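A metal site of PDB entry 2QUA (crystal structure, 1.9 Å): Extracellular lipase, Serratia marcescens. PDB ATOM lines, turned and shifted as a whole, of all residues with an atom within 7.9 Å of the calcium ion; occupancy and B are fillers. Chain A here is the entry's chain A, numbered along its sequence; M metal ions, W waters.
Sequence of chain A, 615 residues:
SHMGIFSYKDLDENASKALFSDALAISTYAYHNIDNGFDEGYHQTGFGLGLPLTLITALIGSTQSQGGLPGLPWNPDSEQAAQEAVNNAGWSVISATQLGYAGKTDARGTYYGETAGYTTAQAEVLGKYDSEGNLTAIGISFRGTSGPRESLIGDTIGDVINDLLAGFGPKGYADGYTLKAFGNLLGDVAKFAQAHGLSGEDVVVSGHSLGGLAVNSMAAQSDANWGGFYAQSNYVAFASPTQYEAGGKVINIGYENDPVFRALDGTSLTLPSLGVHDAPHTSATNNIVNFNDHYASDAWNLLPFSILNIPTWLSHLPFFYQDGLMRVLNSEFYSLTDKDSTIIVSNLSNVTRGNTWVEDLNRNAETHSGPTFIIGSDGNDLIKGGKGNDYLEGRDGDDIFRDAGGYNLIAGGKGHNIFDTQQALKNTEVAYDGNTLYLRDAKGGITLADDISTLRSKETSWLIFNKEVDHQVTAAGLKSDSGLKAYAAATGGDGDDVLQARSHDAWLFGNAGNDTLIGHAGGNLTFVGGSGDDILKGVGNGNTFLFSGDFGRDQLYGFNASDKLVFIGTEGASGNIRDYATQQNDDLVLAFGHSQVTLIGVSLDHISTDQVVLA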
ATOM      1  N   TYR A 112     -36.193  13.850  12.211  1.00  0.00           N
ATOM      2  CA  TYR A 112     -35.680  14.537  13.413  1.00  0.00           C
ATOM      3  C   TYR A 112     -35.676  13.647  14.658  1.00  0.00           C
ATOM      4  O   TYR A 112     -36.544  12.784  14.817  1.00  0.00           O
ATOM      5  CB  TYR A 112     -36.517  15.797  13.689  1.00  0.00           C
ATOM      6  CG  TYR A 112     -36.277  16.919  12.707  1.00  0.00           C
ATOM      7  CD1 TYR A 112     -35.783  18.158  13.143  1.00  0.00           C
ATOM      8  CD2 TYR A 112     -36.555  16.758  11.344  1.00  0.00           C
ATOM      9  CE1 TYR A 112     -35.556  19.194  12.223  1.00  0.00           C
ATOM     10  CE2 TYR A 112     -36.336  17.767  10.437  1.00  0.00           C
ATOM     11  CZ  TYR A 112     -35.838  18.987  10.884  1.00  0.00           C
ATOM     12  OH  TYR A 112     -35.635  19.995   9.968  1.00  0.00           O
ATOM     13  N   TYR A 118     -32.427  15.261  22.067  1.00  0.00           N
ATOM     14  CA  TYR A 118     -31.939  14.716  20.822  1.00  0.00           C
ATOM     15  C   TYR A 118     -32.743  15.269  19.643  1.00  0.00           C
ATOM     16  O   TYR A 118     -32.597  14.797  18.528  1.00  0.00           O
ATOM     17  CB  TYR A 118     -32.033  13.187  20.842  1.00  0.00           C
ATOM     18  CG  TYR A 118     -31.224  12.576  21.971  1.00  0.00           C
ATOM     19  CD1 TYR A 118     -29.911  12.197  21.763  1.00  0.00           C
ATOM     20  CD2 TYR A 118     -31.787  12.399  23.240  1.00  0.00           C
ATOM     21  CE1 TYR A 118     -29.159  11.650  22.778  1.00  0.00           C
ATOM     22  CE2 TYR A 118     -31.032  11.847  24.263  1.00  0.00           C
ATOM     23  CZ  TYR A 118     -29.716  11.477  24.011  1.00  0.00           C
ATOM     24  OH  TYR A 118     -28.924  10.922  24.993  1.00  0.00           O
ATOM     25  N   THR A 119     -33.592  16.260  19.929  1.00  0.00           N
ATOM     26  CA  THR A 119     -34.528  16.751  18.913  1.00  0.00           C
ATOM     27  C   THR A 119     -33.863  17.579  17.815  1.00  0.00           C
ATOM     28  O   THR A 119     -34.517  17.921  16.818  1.00  0.00           O
ATOM     29  CB  THR A 119     -35.662  17.605  19.548  1.00  0.00           C
ATOM     30  OG1 THR A 119     -35.090  18.692  20.282  1.00  0.00           O
ATOM     31  CG2 THR A 119     -36.535  16.764  20.484  1.00  0.00           C
ATOM     32  N   THR A 120     -32.575  17.901  17.971  1.00  0.00           N
ATOM     33  CA  THR A 120     -31.847  18.590  16.897  1.00  0.00           C
ATOM     34  C   THR A 120     -31.015  17.582  16.096  1.00  0.00           C
ATOM     35  O   THR A 120     -30.228  17.967  15.244  1.00  0.00           O
ATOM     36  CB  THR A 120     -30.932  19.761  17.399  1.00  0.00           C
ATOM     37  OG1 THR A 120     -29.835  19.257  18.169  1.00  0.00           O
ATOM     38  CG2 THR A 120     -31.703  20.767  18.211  1.00  0.00           C
ATOM     39  N   ALA A 121     -31.186  16.298  16.377  1.00  0.00           N
ATOM     40  CA  ALA A 121     -30.573  15.265  15.560  1.00  0.00           C
ATOM     41  C   ALA A 121     -31.317  15.162  14.230  1.00  0.00           C
ATOM     42  O   ALA A 121     -32.535  15.307  14.167  1.00  0.00           O
ATOM     43  CB  ALA A 121     -30.619  13.898  16.299  1.00  0.00           C
ATOM     44  N   GLN A 122     -30.577  14.877  13.162  1.00  0.00           N
ATOM     45  CA  GLN A 122     -31.186  14.708  11.850  1.00  0.00           C
ATOM     46  C   GLN A 122     -30.715  13.409  11.195  1.00  0.00           C
ATOM     47  O   GLN A 122     -29.527  13.022  11.318  1.00  0.00           O
ATOM     48  CB  GLN A 122     -30.875  15.901  10.909  1.00  0.00           C
ATOM     49  CG  GLN A 122     -31.738  17.125  11.111  1.00  0.00           C
ATOM     50  CD  GLN A 122     -31.199  18.088  12.165  1.00  0.00           C
ATOM     51  OE1 GLN A 122     -29.974  18.231  12.346  1.00  0.00           O
ATOM     52  NE2 GLN A 122     -32.127  18.763  12.856  1.00  0.00           N
ATOM     53  N   ALA A 123     -31.639  12.738  10.514  1.00  0.00           N
ATOM     54  CA  ALA A 123     -31.273  11.525   9.780  1.00  0.00           C
ATOM     55  C   ALA A 123     -31.925  11.569   8.421  1.00  0.00           C
ATOM     56  O   ALA A 123     -32.969  12.215   8.242  1.00  0.00           O
ATOM     57  CB  ALA A 123     -31.695  10.272  10.540  1.00  0.00           C
ATOM     58  N   ARG A 143     -26.854  13.195  10.287  1.00  0.00           N
ATOM     59  CA  ARG A 143     -26.192  14.483  10.115  1.00  0.00           C
ATOM     60  C   ARG A 143     -25.168  14.780  11.219  1.00  0.00           C
ATOM     61  O   ARG A 143     -25.403  14.473  12.389  1.00  0.00           O
ATOM     62  CB  ARG A 143     -27.221  15.616  10.001  1.00  0.00           C
ATOM     63  CG  ARG A 143     -26.576  16.959   9.683  1.00  0.00           C
ATOM     64  CD  ARG A 143     -27.610  18.065   9.466  1.00  0.00           C
ATOM     65  NE  ARG A 143     -26.924  19.280   9.027  1.00  0.00           N
ATOM     66  CZ  ARG A 143     -27.405  20.175   8.161  1.00  0.00           C
ATOM     67  NH1 ARG A 143     -28.600  20.042   7.588  1.00  0.00           N
ATOM     68  NH2 ARG A 143     -26.660  21.231   7.860  1.00  0.00           N
ATOM     69  N   GLY A 144     -24.055  15.409  10.853  1.00  0.00           N
ATOM     70  CA  GLY A 144     -23.096  15.915  11.840  1.00  0.00           C
ATOM     71  C   GLY A 144     -23.654  17.180  12.458  1.00  0.00           C
ATOM     72  O   GLY A 144     -24.828  17.467  12.316  1.00  0.00           O
ATOM     73  N   THR A 145     -22.807  17.931  13.145  1.00  0.00           N
ATOM     74  CA  THR A 145     -23.261  19.166  13.778  1.00  0.00           C
ATOM     75  C   THR A 145     -23.744  20.209  12.756  1.00  0.00           C
ATOM     76  O   THR A 145     -23.076  20.467  11.746  1.00  0.00           O
ATOM     77  CB  THR A 145     -22.163  19.758  14.665  1.00  0.00           C
ATOM     78  OG1 THR A 145     -21.918  18.849  15.740  1.00  0.00           O
ATOM     79  CG2 THR A 145     -22.584  21.098  15.251  1.00  0.00           C
ATOM     80  N   SER A 146     -24.895  20.793  13.055  1.00  0.00           N
ATOM     81  CA  SER A 146     -25.637  21.740  12.212  1.00  0.00           C
ATOM     82  C   SER A 146     -27.013  21.155  11.850  1.00  0.00           C
ATOM     83  O   SER A 146     -27.316  19.984  12.153  1.00  0.00           O
ATOM     84  CB  SER A 146     -24.862  22.190  10.957  1.00  0.00           C
ATOM     85  OG  SER A 146     -24.764  21.162   9.984  1.00  0.00           O
ATOM     86  N   GLY A 147     -27.827  21.975  11.192  1.00  0.00           N
ATOM     87  CA  GLY A 147     -29.199  21.590  10.867  1.00  0.00           C
ATOM     88  C   GLY A 147     -29.626  22.393   9.660  1.00  0.00           C
ATOM     89  O   GLY A 147     -28.820  23.098   9.089  1.00  0.00           O
ATOM     90  N   PRO A 148     -30.910  22.266   9.276  1.00  0.00           N
ATOM     91  CA  PRO A 148     -31.481  23.055   8.191  1.00  0.00           C
ATOM     92  C   PRO A 148     -31.095  24.506   8.343  1.00  0.00           C
ATOM     93  O   PRO A 148     -31.079  25.027   9.462  1.00  0.00           O
ATOM     94  CB  PRO A 148     -32.985  22.947   8.429  1.00  0.00           C
ATOM     95  CG  PRO A 148     -33.185  21.790   9.362  1.00  0.00           C
ATOM     96  CD  PRO A 148     -31.873  21.322   9.870  1.00  0.00           C
ATOM     97  N   SER A 151     -33.009  27.099  10.617  1.00  0.00           N
ATOM     98  CA  SER A 151     -32.946  27.016  12.073  1.00  0.00           C
ATOM     99  C   SER A 151     -31.507  26.692  12.511  1.00  0.00           C
ATOM    100  O   SER A 151     -31.276  26.105  13.557  1.00  0.00           O
ATOM    101  CB  SER A 151     -33.950  25.993  12.596  1.00  0.00           C
ATOM    102  OG  SER A 151     -33.723  24.721  12.005  1.00  0.00           O
ATOM    103  N   LEU A 152     -30.568  27.140  11.687  1.00  0.00           N
ATOM    104  CA  LEU A 152     -29.145  26.781  11.810  1.00  0.00           C
ATOM    105  C   LEU A 152     -28.551  26.972  13.204  1.00  0.00           C
ATOM    106  O   LEU A 152     -27.932  26.051  13.750  1.00  0.00           O
ATOM    107  CB  LEU A 152     -28.310  27.565  10.779  1.00  0.00           C
ATOM    108  CG  LEU A 152     -26.811  27.233  10.677  1.00  0.00           C
ATOM    109  CD1 LEU A 152     -26.577  25.733  10.537  1.00  0.00           C
ATOM    110  CD2 LEU A 152     -26.158  28.027   9.537  1.00  0.00           C
ATOM    111  N   GLY A 154     -29.969  27.665  16.291  1.00  0.00           N
ATOM    112  CA  GLY A 154     -30.620  26.935  17.371  1.00  0.00           C
ATOM    113  C   GLY A 154     -30.339  25.450  17.285  1.00  0.00           C
ATOM    114  O   GLY A 154     -30.073  24.797  18.301  1.00  0.00           O
ATOM    115  N   ASP A 155     -30.394  24.914  16.059  1.00  0.00           N
ATOM    116  CA  ASP A 155     -30.199  23.500  15.864  1.00  0.00           C
ATOM    117  C   ASP A 155     -28.745  23.154  16.220  1.00  0.00           C
ATOM    118  O   ASP A 155     -28.486  22.189  16.930  1.00  0.00           O
ATOM    119  CB  ASP A 155     -30.559  23.089  14.427  1.00  0.00           C
ATOM    120  CG  ASP A 155     -30.600  21.585  14.244  1.00  0.00           C
ATOM    121  OD1 ASP A 155     -29.532  20.985  14.080  1.00  0.00           O
ATOM    122  OD2 ASP A 155     -31.700  20.995  14.268  1.00  0.00           O
ATOM    123  N   THR A 156     -27.812  23.973  15.733  1.00  0.00           N
ATOM    124  CA  THR A 156     -26.391  23.745  15.989  1.00  0.00           C
ATOM    125  C   THR A 156     -26.115  23.710  17.489  1.00  0.00           C
ATOM    126  O   THR A 156     -25.329  22.883  17.967  1.00  0.00           O
ATOM    127  CB  THR A 156     -25.522  24.811  15.283  1.00  0.00           C
ATOM    128  OG1 THR A 156     -25.738  24.738  13.866  1.00  0.00           O
ATOM    129  CG2 THR A 156     -24.029  24.601  15.572  1.00  0.00           C
ATOM    130  N   ILE A 157     -26.766  24.595  18.254  1.00  0.00           N
ATOM    131  CA  ILE A 157     -26.567  24.628  19.691  1.00  0.00           C
ATOM    132  C   ILE A 157     -27.007  23.325  20.352  1.00  0.00           C
ATOM    133  O   ILE A 157     -26.318  22.762  21.233  1.00  0.00           O
ATOM    134  CB  ILE A 157     -27.269  25.855  20.317  1.00  0.00           C
ATOM    135  CG1 ILE A 157     -26.468  27.113  19.996  1.00  0.00           C
ATOM    136  CG2 ILE A 157     -27.478  25.699  21.845  1.00  0.00           C
ATOM    137  CD1 ILE A 157     -27.214  28.401  20.341  1.00  0.00           C
ATOM    138  N   GLY A 158     -28.165  22.819  19.941  1.00  0.00           N
ATOM    139  CA  GLY A 158     -28.608  21.513  20.402  1.00  0.00           C
ATOM    140  C   GLY A 158     -27.532  20.468  20.142  1.00  0.00           C
ATOM    141  O   GLY A 158     -27.200  19.688  21.040  1.00  0.00           O
ATOM    142  N   ASP A 159     -27.000  20.445  18.922  1.00  0.00           N
ATOM    143  CA  ASP A 159     -25.971  19.463  18.521  1.00  0.00           C
ATOM    144  C   ASP A 159     -24.691  19.576  19.358  1.00  0.00           C
ATOM    145  O   ASP A 159     -24.146  18.576  19.784  1.00  0.00           O
ATOM    146  CB  ASP A 159     -25.571  19.610  17.048  1.00  0.00           C
ATOM    147  CG  ASP A 159     -26.736  19.398  16.052  1.00  0.00           C
ATOM    148  OD1 ASP A 159     -27.736  18.700  16.318  1.00  0.00           O
ATOM    149  OD2 ASP A 159     -26.629  19.943  14.934  1.00  0.00           O
ATOM    150  N   VAL A 160     -24.221  20.805  19.573  1.00  0.00           N
ATOM    151  CA  VAL A 160     -23.056  21.057  20.394  1.00  0.00           C
ATOM    152  C   VAL A 160     -23.242  20.513  21.819  1.00  0.00           C
ATOM    153  O   VAL A 160     -22.290  20.003  22.418  1.00  0.00           O
ATOM    154  CB  VAL A 160     -22.701  22.559  20.441  1.00  0.00           C
ATOM    155  CG1 VAL A 160     -21.637  22.835  21.516  1.00  0.00           C
ATOM    156  CG2 VAL A 160     -22.236  23.048  19.057  1.00  0.00           C
ATOM    157  N   ASN A 162     -25.010  17.889  22.557  1.00  0.00           N
ATOM    158  CA  ASN A 162     -24.830  16.445  22.361  1.00  0.00           C
ATOM    159  C   ASN A 162     -23.348  16.090  22.202  1.00  0.00           C
ATOM    160  O   ASN A 162     -22.899  15.067  22.714  1.00  0.00           O
ATOM    161  CB  ASN A 162     -25.606  15.946  21.145  1.00  0.00           C
ATOM    162  CG  ASN A 162     -27.118  16.034  21.322  1.00  0.00           C
ATOM    163  OD1 ASN A 162     -27.843  16.289  20.360  1.00  0.00           O
ATOM    164  ND2 ASN A 162     -27.587  15.816  22.541  1.00  0.00           N
ATOM    165  N   TYR A 177     -26.714   7.516  21.815  1.00  0.00           N
ATOM    166  CA  TYR A 177     -27.170   8.645  21.000  1.00  0.00           C
ATOM    167  C   TYR A 177     -28.191   8.211  19.958  1.00  0.00           C
ATOM    168  O   TYR A 177     -29.278   8.792  19.867  1.00  0.00           O
ATOM    169  CB  TYR A 177     -25.991   9.372  20.346  1.00  0.00           C
ATOM    170  CG  TYR A 177     -26.385  10.525  19.420  1.00  0.00           C
ATOM    171  CD1 TYR A 177     -26.637  11.812  19.906  1.00  0.00           C
ATOM    172  CD2 TYR A 177     -26.505  10.314  18.052  1.00  0.00           C
ATOM    173  CE1 TYR A 177     -26.995  12.855  19.035  1.00  0.00           C
ATOM    174  CE2 TYR A 177     -26.863  11.344  17.184  1.00  0.00           C
ATOM    175  CZ  TYR A 177     -27.096  12.602  17.670  1.00  0.00           C
ATOM    176  OH  TYR A 177     -27.441  13.586  16.768  1.00  0.00           O
ATOM    177  N   LEU A 210     -20.522  14.276  14.204  1.00  0.00           N
ATOM    178  CA  LEU A 210     -21.514  13.764  15.144  1.00  0.00           C
ATOM    179  C   LEU A 210     -22.303  12.674  14.420  1.00  0.00           C
ATOM    180  O   LEU A 210     -22.737  11.705  15.039  1.00  0.00           O
ATOM    181  CB  LEU A 210     -22.407  14.899  15.663  1.00  0.00           C
ATOM    182  CG  LEU A 210     -23.651  14.572  16.494  1.00  0.00           C
ATOM    183  CD1 LEU A 210     -23.310  13.876  17.803  1.00  0.00           C
ATOM    184  CD2 LEU A 210     -24.461  15.856  16.750  1.00  0.00           C
HETATM  185 CA    CA M   1     -28.507  18.969  14.001  1.00  0.00          CA
HETATM  186  O   HOH W   1     -27.250  17.059  13.487  1.00  0.00           O
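Five residues have an atom within 4 Å of the calcium ion: Thr 120, Gln 122, Ser 146, Asp 155 and Asp 159.
Along chain A the residues within 4 Å of the calcium ion span positions 120 to 159.
The nearest printed residue that does not touch the calcium ion is Gly 147 (4.1 Å).
The calcium ion is bound by the side-chain carboxylate (OD1) of Asp 155 (2.3 Å), the side-chain carboxylate (OD2) of Asp 159 (2.3 Å), the side-chain amide oxygen (OE1) of Gln 122 (2.3 Å), water W1 (2.3 Å), the backbone carbonyl oxygen (O) of Thr 120 (2.3 Å), the backbone carbonyl oxygen (O) of Ser 146 (2.4 Å) and the side-chain carboxylate (OD1) of Asp 159 (2.5 Å).
The calcium ion has seven donor atoms within binding distance.
O of Gln 122 sits at hydrogen-bond distance from N of Arg 143 (2.9 Å).
The side-chain hydroxyl of Ser 146 is in hydrogen-bond range of the guanidinium group of Arg 143 (2.8 Å).
The side-chain carboxylate (OD1) of Asp 155 lies close to the backbone NH (N) of Gly 147 (3.5 Å).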
